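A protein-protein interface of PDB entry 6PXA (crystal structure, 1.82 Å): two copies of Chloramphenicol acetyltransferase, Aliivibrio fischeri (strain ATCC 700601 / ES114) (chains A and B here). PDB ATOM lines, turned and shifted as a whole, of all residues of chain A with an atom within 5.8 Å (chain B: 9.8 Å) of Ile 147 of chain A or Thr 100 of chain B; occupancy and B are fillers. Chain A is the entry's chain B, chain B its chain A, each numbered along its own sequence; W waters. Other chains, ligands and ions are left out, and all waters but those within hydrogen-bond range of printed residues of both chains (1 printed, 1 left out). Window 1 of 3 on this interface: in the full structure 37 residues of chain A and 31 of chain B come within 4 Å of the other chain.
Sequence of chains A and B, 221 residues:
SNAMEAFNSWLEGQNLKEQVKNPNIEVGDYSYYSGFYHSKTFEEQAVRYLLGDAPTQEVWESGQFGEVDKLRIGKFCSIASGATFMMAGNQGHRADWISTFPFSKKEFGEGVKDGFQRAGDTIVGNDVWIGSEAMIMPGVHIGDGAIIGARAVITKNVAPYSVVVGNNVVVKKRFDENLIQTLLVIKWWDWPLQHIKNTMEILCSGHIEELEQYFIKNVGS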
ATOM      1  N   PHE A  76      21.116  18.165   6.204  1.00  0.00           N
ATOM      2  CA  PHE A  76      21.421  17.779   7.574  1.00  0.00           C
ATOM      3  C   PHE A  76      21.246  18.939   8.547  1.00  0.00           C
ATOM      4  O   PHE A  76      21.987  19.055   9.532  1.00  0.00           O
ATOM      5  CB  PHE A  76      22.830  17.210   7.661  1.00  0.00           C
ATOM      6  CG  PHE A  76      22.981  15.882   6.971  1.00  0.00           C
ATOM      7  CD1 PHE A  76      22.303  14.777   7.428  1.00  0.00           C
ATOM      8  CD2 PHE A  76      23.778  15.745   5.843  1.00  0.00           C
ATOM      9  CE1 PHE A  76      22.434  13.541   6.791  1.00  0.00           C
ATOM     10  CE2 PHE A  76      23.916  14.505   5.209  1.00  0.00           C
ATOM     11  CZ  PHE A  76      23.238  13.412   5.683  1.00  0.00           C
ATOM     12  N   SER A  78      19.013  21.149  11.295  1.00  0.00           N
ATOM     13  CA  SER A  78      18.049  20.931  12.373  1.00  0.00           C
ATOM     14  C   SER A  78      17.427  22.276  12.674  1.00  0.00           C
ATOM     15  O   SER A  78      18.118  23.181  13.148  1.00  0.00           O
ATOM     16  CB  SER A  78      18.715  20.353  13.624  1.00  0.00           C
ATOM     17  OG  SER A  78      19.267  19.073  13.347  1.00  0.00           O
ATOM     18  N   ASP A 127      24.581  21.066   7.840  1.00  0.00           N
ATOM     19  CA  ASP A 127      24.839  20.692   9.221  1.00  0.00           C
ATOM     20  C   ASP A 127      24.676  21.898  10.153  1.00  0.00           C
ATOM     21  O   ASP A 127      25.506  22.153  11.026  1.00  0.00           O
ATOM     22  CB  ASP A 127      26.229  20.067   9.364  1.00  0.00           C
ATOM     23  CG  ASP A 127      26.482  19.551  10.787  1.00  0.00           C
ATOM     24  OD1 ASP A 127      25.560  18.936  11.361  1.00  0.00           O
ATOM     25  OD2 ASP A 127      27.575  19.788  11.341  1.00  0.00           O
ATOM     26  N   VAL A 128      23.601  22.654   9.954  1.00  0.00           N
ATOM     27  CA  VAL A 128      23.332  23.855  10.748  1.00  0.00           C
ATOM     28  C   VAL A 128      22.159  23.589  11.667  1.00  0.00           C
ATOM     29  O   VAL A 128      21.123  23.065  11.238  1.00  0.00           O
ATOM     30  CB  VAL A 128      23.077  25.082   9.846  1.00  0.00           C
ATOM     31  CG1 VAL A 128      22.587  26.280  10.675  1.00  0.00           C
ATOM     32  CG2 VAL A 128      24.332  25.447   9.093  1.00  0.00           C
ATOM     33  N   TRP A 129      22.357  23.877  12.953  1.00  0.00           N
ATOM     34  CA  TRP A 129      21.352  23.724  13.995  1.00  0.00           C
ATOM     35  C   TRP A 129      20.832  25.112  14.345  1.00  0.00           C
ATOM     36  O   TRP A 129      21.614  25.981  14.744  1.00  0.00           O
ATOM     37  CB  TRP A 129      21.973  23.047  15.215  1.00  0.00           C
ATOM     38  CG  TRP A 129      21.085  22.877  16.411  1.00  0.00           C
ATOM     39  CD1 TRP A 129      19.722  22.789  16.437  1.00  0.00           C
ATOM     40  CD2 TRP A 129      21.524  22.751  17.763  1.00  0.00           C
ATOM     41  NE1 TRP A 129      19.281  22.633  17.742  1.00  0.00           N
ATOM     42  CE2 TRP A 129      20.371  22.595  18.568  1.00  0.00           C
ATOM     43  CE3 TRP A 129      22.782  22.765  18.376  1.00  0.00           C
ATOM     44  CZ2 TRP A 129      20.441  22.464  19.950  1.00  0.00           C
ATOM     45  CZ3 TRP A 129      22.842  22.633  19.757  1.00  0.00           C
ATOM     46  CH2 TRP A 129      21.681  22.490  20.519  1.00  0.00           C
ATOM     47  N   ILE A 130      19.530  25.323  14.172  1.00  0.00           N
ATOM     48  CA  ILE A 130      18.895  26.629  14.388  1.00  0.00           C
ATOM     49  C   ILE A 130      17.906  26.483  15.537  1.00  0.00           C
ATOM     50  O   ILE A 130      16.850  25.851  15.392  1.00  0.00           O
ATOM     51  CB  ILE A 130      18.202  27.169  13.120  1.00  0.00           C
ATOM     52  CG1 ILE A 130      19.207  27.300  11.965  1.00  0.00           C
ATOM     53  CG2 ILE A 130      17.495  28.509  13.401  1.00  0.00           C
ATOM     54  CD1 ILE A 130      18.613  27.822  10.692  1.00  0.00           C
ATOM     55  N   GLY A 145      27.882  24.012   9.499  1.00  0.00           N
ATOM     56  CA  GLY A 145      28.241  23.654  10.858  1.00  0.00           C
ATOM     57  C   GLY A 145      27.921  24.683  11.926  1.00  0.00           C
ATOM     58  O   GLY A 145      28.244  24.446  13.099  1.00  0.00           O
ATOM     59  N   ALA A 146      27.321  25.819  11.572  1.00  0.00           N
ATOM     60  CA  ALA A 146      27.017  26.816  12.594  1.00  0.00           C
ATOM     61  C   ALA A 146      25.906  26.356  13.542  1.00  0.00           C
ATOM     62  O   ALA A 146      25.104  25.466  13.240  1.00  0.00           O
ATOM     63  CB  ALA A 146      26.603  28.145  11.958  1.00  0.00           C
ATOM     64  N   ILE A 147      25.859  26.993  14.712  1.00  0.00           N
ATOM     65  CA  ILE A 147      24.770  26.814  15.664  1.00  0.00           C
ATOM     66  C   ILE A 147      24.207  28.189  15.953  1.00  0.00           C
ATOM     67  O   ILE A 147      24.963  29.102  16.301  1.00  0.00           O
ATOM     68  CB  ILE A 147      25.226  26.132  16.970  1.00  0.00           C
ATOM     69  CG1 ILE A 147      25.693  24.704  16.687  1.00  0.00           C
ATOM     70  CG2 ILE A 147      24.106  26.089  17.976  1.00  0.00           C
ATOM     71  CD1 ILE A 147      26.450  24.101  17.824  1.00  0.00           C
ATOM     72  N   ILE A 148      22.907  28.348  15.744  1.00  0.00           N
ATOM     73  CA  ILE A 148      22.201  29.577  16.047  1.00  0.00           C
ATOM     74  C   ILE A 148      21.432  29.338  17.349  1.00  0.00           C
ATOM     75  O   ILE A 148      20.624  28.403  17.450  1.00  0.00           O
ATOM     76  CB  ILE A 148      21.251  29.998  14.913  1.00  0.00           C
ATOM     77  CG1 ILE A 148      21.987  30.151  13.577  1.00  0.00           C
ATOM     78  CG2 ILE A 148      20.525  31.313  15.278  1.00  0.00           C
ATOM     79  CD1 ILE A 148      23.260  31.020  13.653  1.00  0.00           C
ATOM     80  N   GLY A 149      21.694  30.165  18.347  1.00  0.00           N
ATOM     81  CA  GLY A 149      21.046  29.974  19.639  1.00  0.00           C
ATOM     82  C   GLY A 149      19.557  30.244  19.583  1.00  0.00           C
ATOM     83  O   GLY A 149      19.058  30.983  18.722  1.00  0.00           O
ATOM     84  N   VAL A 158      27.181  34.408   9.225  1.00  0.00           N
ATOM     85  CA  VAL A 158      27.704  33.574  10.310  1.00  0.00           C
ATOM     86  C   VAL A 158      28.774  32.657   9.728  1.00  0.00           C
ATOM     87  O   VAL A 158      28.500  31.885   8.799  1.00  0.00           O
ATOM     88  CB  VAL A 158      26.576  32.777  10.989  1.00  0.00           C
ATOM     89  CG1 VAL A 158      27.124  31.785  12.014  1.00  0.00           C
ATOM     90  CG2 VAL A 158      25.598  33.741  11.653  1.00  0.00           C
ATOM     91  N   TYR A 161      30.824  26.861  11.492  1.00  0.00           N
ATOM     92  CA  TYR A 161      31.085  26.260  12.801  1.00  0.00           C
ATOM     93  C   TYR A 161      31.144  27.294  13.920  1.00  0.00           C
ATOM     94  O   TYR A 161      31.702  27.020  14.996  1.00  0.00           O
ATOM     95  CB  TYR A 161      32.356  25.410  12.765  1.00  0.00           C
ATOM     96  CG  TYR A 161      32.146  24.175  11.933  1.00  0.00           C
ATOM     97  CD1 TYR A 161      31.549  23.043  12.474  1.00  0.00           C
ATOM     98  CD2 TYR A 161      32.492  24.160  10.591  1.00  0.00           C
ATOM     99  CE1 TYR A 161      31.332  21.917  11.707  1.00  0.00           C
ATOM    100  CE2 TYR A 161      32.275  23.050   9.812  1.00  0.00           C
ATOM    101  CZ  TYR A 161      31.692  21.939  10.371  1.00  0.00           C
ATOM    102  OH  TYR A 161      31.486  20.856   9.571  1.00  0.00           O
ATOM    103  N   SER A 162      30.574  28.474  13.672  1.00  0.00           N
ATOM    104  CA  SER A 162      30.350  29.465  14.712  1.00  0.00           C
ATOM    105  C   SER A 162      29.107  29.130  15.542  1.00  0.00           C
ATOM    106  O   SER A 162      28.123  28.566  15.042  1.00  0.00           O
ATOM    107  CB  SER A 162      30.195  30.857  14.081  1.00  0.00           C
ATOM    108  OG  SER A 162      31.447  31.382  13.675  1.00  0.00           O
ATOM    109  N   VAL A 163      29.141  29.518  16.818  1.00  0.00           N
ATOM    110  CA  VAL A 163      27.962  29.513  17.684  1.00  0.00           C
ATOM    111  C   VAL A 163      27.565  30.960  17.958  1.00  0.00           C
ATOM    112  O   VAL A 163      28.370  31.742  18.479  1.00  0.00           O
ATOM    113  CB  VAL A 163      28.239  28.771  19.001  1.00  0.00           C
ATOM    114  CG1 VAL A 163      26.959  28.667  19.854  1.00  0.00           C
ATOM    115  CG2 VAL A 163      28.845  27.420  18.722  1.00  0.00           C
ATOM    116  N   VAL A 164      26.321  31.313  17.642  1.00  0.00           N
ATOM    117  CA  VAL A 164      25.883  32.710  17.660  1.00  0.00           C
ATOM    118  C   VAL A 164      24.576  32.796  18.429  1.00  0.00           C
ATOM    119  O   VAL A 164      23.649  32.020  18.175  1.00  0.00           O
ATOM    120  CB  VAL A 164      25.724  33.290  16.238  1.00  0.00           C
ATOM    121  CG1 VAL A 164      25.521  34.831  16.265  1.00  0.00           C
ATOM    122  CG2 VAL A 164      26.929  32.920  15.370  1.00  0.00           C
ATOM    123  N   VAL A 165      24.506  33.733  19.371  1.00  0.00           N
ATOM    124  CA  VAL A 165      23.306  33.949  20.175  1.00  0.00           C
ATOM    125  C   VAL A 165      22.958  35.433  20.156  1.00  0.00           C
ATOM    126  O   VAL A 165      23.769  36.280  19.790  1.00  0.00           O
ATOM    127  CB  VAL A 165      23.462  33.481  21.645  1.00  0.00           C
ATOM    128  CG1 VAL A 165      23.927  32.032  21.718  1.00  0.00           C
ATOM    129  CG2 VAL A 165      24.498  34.340  22.365  1.00  0.00           C
ATOM    130  N   ARG A 174      33.028  25.867  17.243  1.00  0.00           N
ATOM    131  CA  ARG A 174      32.899  24.511  17.783  1.00  0.00           C
ATOM    132  C   ARG A 174      34.242  23.797  17.829  1.00  0.00           C
ATOM    133  O   ARG A 174      34.484  22.988  18.732  1.00  0.00           O
ATOM    134  CB  ARG A 174      31.897  23.704  16.957  1.00  0.00           C
ATOM    135  CG  ARG A 174      30.433  24.146  17.093  1.00  0.00           C
ATOM    136  CD  ARG A 174      29.567  23.543  15.991  1.00  0.00           C
ATOM    137  NE  ARG A 174      29.468  22.087  16.079  1.00  0.00           N
ATOM    138  CZ  ARG A 174      29.105  21.286  15.076  1.00  0.00           C
ATOM    139  NH1 ARG A 174      28.805  21.769  13.877  1.00  0.00           N
ATOM    140  NH2 ARG A 174      29.050  19.979  15.268  1.00  0.00           N
ATOM    141  N   ASN B  90      20.137  19.117  25.800  1.00  0.00           N
ATOM    142  CA  ASN B  90      20.548  19.463  24.443  1.00  0.00           C
ATOM    143  C   ASN B  90      19.645  18.853  23.377  1.00  0.00           C
ATOM    144  O   ASN B  90      19.930  19.009  22.184  1.00  0.00           O
ATOM    145  CB  ASN B  90      22.013  19.057  24.217  1.00  0.00           C
ATOM    146  CG  ASN B  90      22.245  17.538  24.280  1.00  0.00           C
ATOM    147  OD1 ASN B  90      21.311  16.748  24.410  1.00  0.00           O
ATOM    148  ND2 ASN B  90      23.506  17.133  24.166  1.00  0.00           N
ATOM    149  N   GLN B  91      18.561  18.175  23.770  1.00  0.00           N
ATOM    150  CA  GLN B  91      17.638  17.534  22.824  1.00  0.00           C
ATOM    151  C   GLN B  91      18.387  16.686  21.803  1.00  0.00           C
ATOM    152  O   GLN B  91      17.958  16.542  20.656  1.00  0.00           O
ATOM    153  CB  GLN B  91      16.747  18.564  22.114  1.00  0.00           C
ATOM    154  CG  GLN B  91      15.928  19.401  23.060  1.00  0.00           C
ATOM    155  CD  GLN B  91      14.841  20.253  22.394  1.00  0.00           C
ATOM    156  OE1 GLN B  91      14.327  19.921  21.325  1.00  0.00           O
ATOM    157  NE2 GLN B  91      14.484  21.360  23.049  1.00  0.00           N
ATOM    158  N   GLY B  92      19.523  16.128  22.214  1.00  0.00           N
ATOM    159  CA  GLY B  92      20.268  15.219  21.375  1.00  0.00           C
ATOM    160  C   GLY B  92      21.305  15.846  20.468  1.00  0.00           C
ATOM    161  O   GLY B  92      22.038  15.097  19.808  1.00  0.00           O
ATOM    162  N   HIS B  93      21.410  17.184  20.421  1.00  0.00           N
ATOM    163  CA  HIS B  93      22.413  17.850  19.590  1.00  0.00           C
ATOM    164  C   HIS B  93      23.677  18.094  20.405  1.00  0.00           C
ATOM    165  O   HIS B  93      23.622  18.729  21.469  1.00  0.00           O
ATOM    166  CB  HIS B  93      21.886  19.173  19.043  1.00  0.00           C
ATOM    167  CG  HIS B  93      20.530  19.059  18.421  1.00  0.00           C
ATOM    168  ND1 HIS B  93      20.342  18.686  17.107  1.00  0.00           N
ATOM    169  CD2 HIS B  93      19.295  19.275  18.933  1.00  0.00           C
ATOM    170  CE1 HIS B  93      19.049  18.669  16.838  1.00  0.00           C
ATOM    171  NE2 HIS B  93      18.392  19.030  17.928  1.00  0.00           N
ATOM    172  N   ARG B  94      24.810  17.603  19.899  1.00  0.00           N
ATOM    173  CA  ARG B  94      26.095  17.693  20.590  1.00  0.00           C
ATOM    174  C   ARG B  94      27.034  18.595  19.800  1.00  0.00           C
ATOM    175  O   ARG B  94      27.627  18.161  18.815  1.00  0.00           O
ATOM    176  CB  ARG B  94      26.683  16.299  20.803  1.00  0.00           C
ATOM    177  CG  ARG B  94      26.061  15.664  22.021  1.00  0.00           C
ATOM    178  CD  ARG B  94      26.813  14.473  22.557  1.00  0.00           C
ATOM    179  NE  ARG B  94      28.110  14.817  23.121  1.00  0.00           N
ATOM    180  CZ  ARG B  94      28.703  14.075  24.047  1.00  0.00           C
ATOM    181  NH1 ARG B  94      28.077  12.997  24.490  1.00  0.00           N
ATOM    182  NH2 ARG B  94      29.902  14.400  24.523  1.00  0.00           N
ATOM    183  N   ALA B  95      27.175  19.855  20.230  1.00  0.00           N
ATOM    184  CA  ALA B  95      28.067  20.775  19.517  1.00  0.00           C
ATOM    185  C   ALA B  95      29.506  20.269  19.456  1.00  0.00           C
ATOM    186  O   ALA B  95      30.279  20.705  18.585  1.00  0.00           O
ATOM    187  CB  ALA B  95      28.035  22.144  20.191  1.00  0.00           C
ATOM    188  N   ASP B  96      29.880  19.359  20.360  1.00  0.00           N
ATOM    189  CA  ASP B  96      31.240  18.842  20.452  1.00  0.00           C
ATOM    190  C   ASP B  96      31.464  17.597  19.602  1.00  0.00           C
ATOM    191  O   ASP B  96      32.606  17.156  19.451  1.00  0.00           O
ATOM    192  CB  ASP B  96      31.593  18.545  21.916  1.00  0.00           C
ATOM    193  CG  ASP B  96      30.638  17.560  22.575  1.00  0.00           C
ATOM    194  OD1 ASP B  96      29.446  17.500  22.214  1.00  0.00           O
ATOM    195  OD2 ASP B  96      31.092  16.835  23.479  1.00  0.00           O
ATOM    196  N   TRP B  97      30.407  17.031  19.045  1.00  0.00           N
ATOM    197  CA  TRP B  97      30.526  16.002  18.034  1.00  0.00           C
ATOM    198  C   TRP B  97      30.611  16.655  16.655  1.00  0.00           C
ATOM    199  O   TRP B  97      30.285  17.834  16.480  1.00  0.00           O
ATOM    200  CB  TRP B  97      29.335  15.050  18.118  1.00  0.00           C
ATOM    201  CG  TRP B  97      29.403  14.082  19.266  1.00  0.00           C
ATOM    202  CD1 TRP B  97      30.399  13.965  20.192  1.00  0.00           C
ATOM    203  CD2 TRP B  97      28.434  13.083  19.589  1.00  0.00           C
ATOM    204  NE1 TRP B  97      30.115  12.938  21.070  1.00  0.00           N
ATOM    205  CE2 TRP B  97      28.910  12.385  20.719  1.00  0.00           C
ATOM    206  CE3 TRP B  97      27.217  12.698  19.019  1.00  0.00           C
ATOM    207  CZ2 TRP B  97      28.212  11.324  21.282  1.00  0.00           C
ATOM    208  CZ3 TRP B  97      26.517  11.667  19.589  1.00  0.00           C
ATOM    209  CH2 TRP B  97      27.015  10.985  20.709  1.00  0.00           C
ATOM    210  N   ILE B  98      31.051  15.866  15.677  1.00  0.00           N
ATOM    211  CA  ILE B  98      31.274  16.378  14.322  1.00  0.00           C
ATOM    212  C   ILE B  98      30.007  17.012  13.761  1.00  0.00           C
ATOM    213  O   ILE B  98      30.032  18.142  13.261  1.00  0.00           O
ATOM    214  CB  ILE B  98      31.799  15.263  13.404  1.00  0.00           C
ATOM    215  CG1 ILE B  98      33.240  14.918  13.771  1.00  0.00           C
ATOM    216  CG2 ILE B  98      31.748  15.711  11.977  1.00  0.00           C
ATOM    217  CD1 ILE B  98      33.819  13.780  12.951  1.00  0.00           C
ATOM    218  N   SER B  99      28.884  16.307  13.837  1.00  0.00           N
ATOM    219  CA  SER B  99      27.603  16.861  13.417  1.00  0.00           C
ATOM    220  C   SER B  99      26.669  17.088  14.603  1.00  0.00           C
ATOM    221  O   SER B  99      26.684  16.330  15.586  1.00  0.00           O
ATOM    222  CB  SER B  99      26.898  15.941  12.424  1.00  0.00           C
ATOM    223  OG  SER B  99      25.582  16.431  12.203  1.00  0.00           O
ATOM    224  N   THR B 100      25.830  18.126  14.495  1.00  0.00           N
ATOM    225  CA  THR B 100      24.721  18.299  15.425  1.00  0.00           C
ATOM    226  C   THR B 100      23.453  17.561  14.992  1.00  0.00           C
ATOM    227  O   THR B 100      22.440  17.636  15.696  1.00  0.00           O
ATOM    228  CB  THR B 100      24.393  19.794  15.626  1.00  0.00           C
ATOM    229  OG1 THR B 100      24.219  20.455  14.361  1.00  0.00           O
ATOM    230  CG2 THR B 100      25.490  20.493  16.455  1.00  0.00           C
ATOM    231  N   PHE B 101      23.478  16.854  13.879  1.00  0.00           N
ATOM    232  CA  PHE B 101      22.245  16.280  13.334  1.00  0.00           C
ATOM    233  C   PHE B 101      21.869  15.012  14.090  1.00  0.00           C
ATOM    234  O   PHE B 101      22.725  14.150  14.297  1.00  0.00           O
ATOM    235  CB  PHE B 101      22.388  15.949  11.851  1.00  0.00           C
ATOM    236  CG  PHE B 101      21.081  15.600  11.181  1.00  0.00           C
ATOM    237  CD1 PHE B 101      20.206  16.602  10.769  1.00  0.00           C
ATOM    238  CD2 PHE B 101      20.710  14.279  11.000  1.00  0.00           C
ATOM    239  CE1 PHE B 101      18.996  16.280  10.161  1.00  0.00           C
ATOM    240  CE2 PHE B 101      19.505  13.954  10.386  1.00  0.00           C
ATOM    241  CZ  PHE B 101      18.651  14.947   9.973  1.00  0.00           C
ATOM    242  N   PRO B 102      20.599  14.847  14.479  1.00  0.00           N
ATOM    243  CA  PRO B 102      20.171  13.620  15.204  1.00  0.00           C
ATOM    244  C   PRO B 102      19.789  12.474  14.273  1.00  0.00           C
ATOM    245  O   PRO B 102      18.621  12.082  14.141  1.00  0.00           O
ATOM    246  CB  PRO B 102      18.990  14.130  16.042  1.00  0.00           C
ATOM    247  CG  PRO B 102      18.409  15.257  15.243  1.00  0.00           C
ATOM    248  CD  PRO B 102      19.540  15.870  14.426  1.00  0.00           C
ATOM    249  N   PHE B 103      20.802  11.913  13.612  1.00  0.00           N
ATOM    250  CA  PHE B 103      20.620  10.762  12.729  1.00  0.00           C
ATOM    251  C   PHE B 103      19.744   9.691  13.381  1.00  0.00           C
ATOM    252  O   PHE B 103      19.989   9.281  14.514  1.00  0.00           O
ATOM    253  CB  PHE B 103      21.979  10.138  12.384  1.00  0.00           C
ATOM    254  CG  PHE B 103      22.999  11.110  11.859  1.00  0.00           C
ATOM    255  CD1 PHE B 103      23.032  11.446  10.506  1.00  0.00           C
ATOM    256  CD2 PHE B 103      23.957  11.651  12.707  1.00  0.00           C
ATOM    257  CE1 PHE B 103      23.979  12.336  10.009  1.00  0.00           C
ATOM    258  CE2 PHE B 103      24.914  12.536  12.222  1.00  0.00           C
ATOM    259  CZ  PHE B 103      24.926  12.878  10.864  1.00  0.00           C
ATOM    260  N   SER B 104      18.731   9.223  12.654  1.00  0.00           N
ATOM    261  CA  SER B 104      17.903   8.138  13.151  1.00  0.00           C
ATOM    262  C   SER B 104      18.531   6.799  12.794  1.00  0.00           C
ATOM    263  O   SER B 104      19.169   6.643  11.747  1.00  0.00           O
ATOM    264  CB  SER B 104      16.475   8.212  12.598  1.00  0.00           C
ATOM    265  OG  SER B 104      16.385   7.796  11.250  1.00  0.00           O
ATOM    266  N   LYS B 113      25.002   6.929  17.519  1.00  0.00           N
ATOM    267  CA  LYS B 113      25.136   7.055  18.967  1.00  0.00           C
ATOM    268  C   LYS B 113      24.212   8.145  19.480  1.00  0.00           C
ATOM    269  O   LYS B 113      24.125   9.231  18.891  1.00  0.00           O
ATOM    270  CB  LYS B 113      26.582   7.375  19.366  1.00  0.00           C
ATOM    271  CG  LYS B 113      27.603   6.398  18.775  1.00  0.00           C
ATOM    272  CD  LYS B 113      28.996   6.601  19.371  1.00  0.00           C
ATOM    273  CE  LYS B 113      29.882   5.384  19.152  1.00  0.00           C
ATOM    274  NZ  LYS B 113      31.222   5.532  19.790  1.00  0.00           N
ATOM    275  N   GLY B 115      23.133  11.175  21.295  1.00  0.00           N
ATOM    276  CA  GLY B 115      23.837  12.342  21.770  1.00  0.00           C
ATOM    277  C   GLY B 115      23.186  13.100  22.914  1.00  0.00           C
ATOM    278  O   GLY B 115      23.719  14.129  23.330  1.00  0.00           O
ATOM    279  N   PHE B 116      22.068  12.614  23.451  1.00  0.00           N
ATOM    280  CA  PHE B 116      21.338  13.339  24.492  1.00  0.00           C
ATOM    281  C   PHE B 116      22.193  13.551  25.737  1.00  0.00           C
ATOM    282  O   PHE B 116      22.930  12.661  26.168  1.00  0.00           O
ATOM    283  CB  PHE B 116      20.067  12.572  24.866  1.00  0.00           C
ATOM    284  CG  PHE B 116      19.289  13.214  25.952  1.00  0.00           C
ATOM    285  CD1 PHE B 116      18.582  14.367  25.716  1.00  0.00           C
ATOM    286  CD2 PHE B 116      19.271  12.668  27.221  1.00  0.00           C
ATOM    287  CE1 PHE B 116      17.860  14.983  26.736  1.00  0.00           C
ATOM    288  CE2 PHE B 116      18.556  13.276  28.234  1.00  0.00           C
ATOM    289  CZ  PHE B 116      17.844  14.434  27.983  1.00  0.00           C
HETATM  290  O   HOH W   1      21.840  19.873  12.432  1.00  0.00           O
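The backbone carbonyl oxygen (O) of Ala 95 of chain B lies within hydrogen-bond range of the guanidinium group (NE) of Arg 174 of chain A (3.0 Å).
The backbone carbonyl oxygen of Trp 97 of chain B sits at hydrogen-bond distance from the guanidinium group of Arg 174 of chain A, at 2.8 Å.
The backbone carbonyl oxygen (O) of Ile 98 of chain B lies within hydrogen-bond range of the guanidinium group (NH2) of Arg 174 of chain A, 2.9 Å away.
OG of Ser 99 of chain B lies within hydrogen-bond range of OD1 of Asp 127 of chain A (2.6 Å).
The side-chain carboxylate (OD1) of Asp 127 of chain A lies within hydrogen-bond range of the backbone NH (N) of Thr 100 of chain B (3.2 Å).
Water W1 lies within hydrogen-bond range of the side-chain hydroxyl (OG) of Ser 78 of chain A (2.8 Å), the backbone carbonyl oxygen (O) of Phe 76 of chain A (3.0 Å), the side-chain hydroxyl (OG1) of Thr 100 of chain B (3.1 Å) and the backbone carbonyl oxygen (O) of Val 128 of chain A (3.5 Å).
Of the 18 printed residues of chain B, 9 touch a printed residue of chain A.
Of the 18 printed residues of chain A, 6 touch a printed residue of chain B.
Printed residues of chain A that touch a printed residue of chain B: Phe 76, Ser 78, Asp 127, Trp 129, Ile 147 and Arg 174.
Hydrophobic or aromatic side chains of chain A within 4 Å of the printed part of chain B: Phe 76, Trp 129 and Ile 147.
No position is printed for both chains.
Of the 18 pairs that touch across the chains among the printed residues, none has its exchanged pair printed and touching as well.
O of Phe 76 of chain A touches CD1 of Phe 101 of chain B (3.3 Å).
Phe 76 of chain A touches Phe 103 of chain B (CE1 to CE1, 3.8 Å).
OG of Ser 78 of chain A touches CD1 of Phe 101 of chain B (3.7 Å).
Asp 127 of chain A touches Ile 98 of chain B.
Asp 127 of chain A touches Phe 101 of chain B (OD1 to N, 3.9 Å).
CB of Trp 129 of chain A touches OG1 of Thr 100 of chain B, at 3.5 Å.
Ile 147 of chain A touches Ala 95 of chain B.
Ile 147 of chain A touches Thr 100 of chain B (CD1 to CG2, 3.98 Å).
Ser 99 of chain B touches Arg 174 of chain A (C to NH2, 3.8 Å).
Thr 100 of chain B touches Arg 174 of chain A (CG2 to NH2, 3.8 Å).
Ile 147 of chain A touches just these residues of chain B: Ala 95 (3.5 Å) and Thr 100 (3.98 Å).
Of the printed residues of chain A, Thr 100 of chain B touches Asp 127, Trp 129, Ile 147 and Arg 174.
No residue of chain B comes within 4 Å of Ala 146 of chain A.
No residue of chain B comes within 4 Å of Ile 148 of chain A.
No residue of chain B comes within 4 Å of Val 163 of chain A.
Of the printed residues of chain B, Arg 174 of chain A touches Ala 95, Trp 97, Ile 98, Ser 99 and Thr 100.
Of the printed residues of chain A, Ala 95 of chain B touches Ile 147 and Arg 174.
Lys 113 of chain B touches none of the printed residues of chain A.
The nearest printed residue of chain A that does not touch Thr 100 of chain B is Ser 78 of chain A (4.2 Å).
The nearest printed residue of chain A that does not touch Phe 103 of chain B is Asp 127 of chain A (6.1 Å).
ND2 of Asn 90 of chain B is in hydrogen-bond range of O of His 93 of chain B, at 3.1 Å.
The backbone carbonyl oxygen (O) of Ser 78 of chain A is in hydrogen-bond range of the backbone NH (N) of Ile 130 of chain A (2.8 Å).
The backbone carbonyl oxygen (O) of Asp 127 of chain A lies close to the backbone NH (N) of Gly 145 of chain A (3.4 Å).
The side-chain carboxylate (OD2) of Asp 127 of chain A lies within salt-bridge range of the guanidinium group (NH1) of Arg 174 of chain A, at 3.4 Å.
N of Ile 147 of chain A sits at hydrogen-bond distance from O of Ser 162 of chain A.
The backbone NH (N) of Val 164 of chain A sits at hydrogen-bond distance from the backbone carbonyl oxygen (O) of Ile 147 of chain A (2.9 Å).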
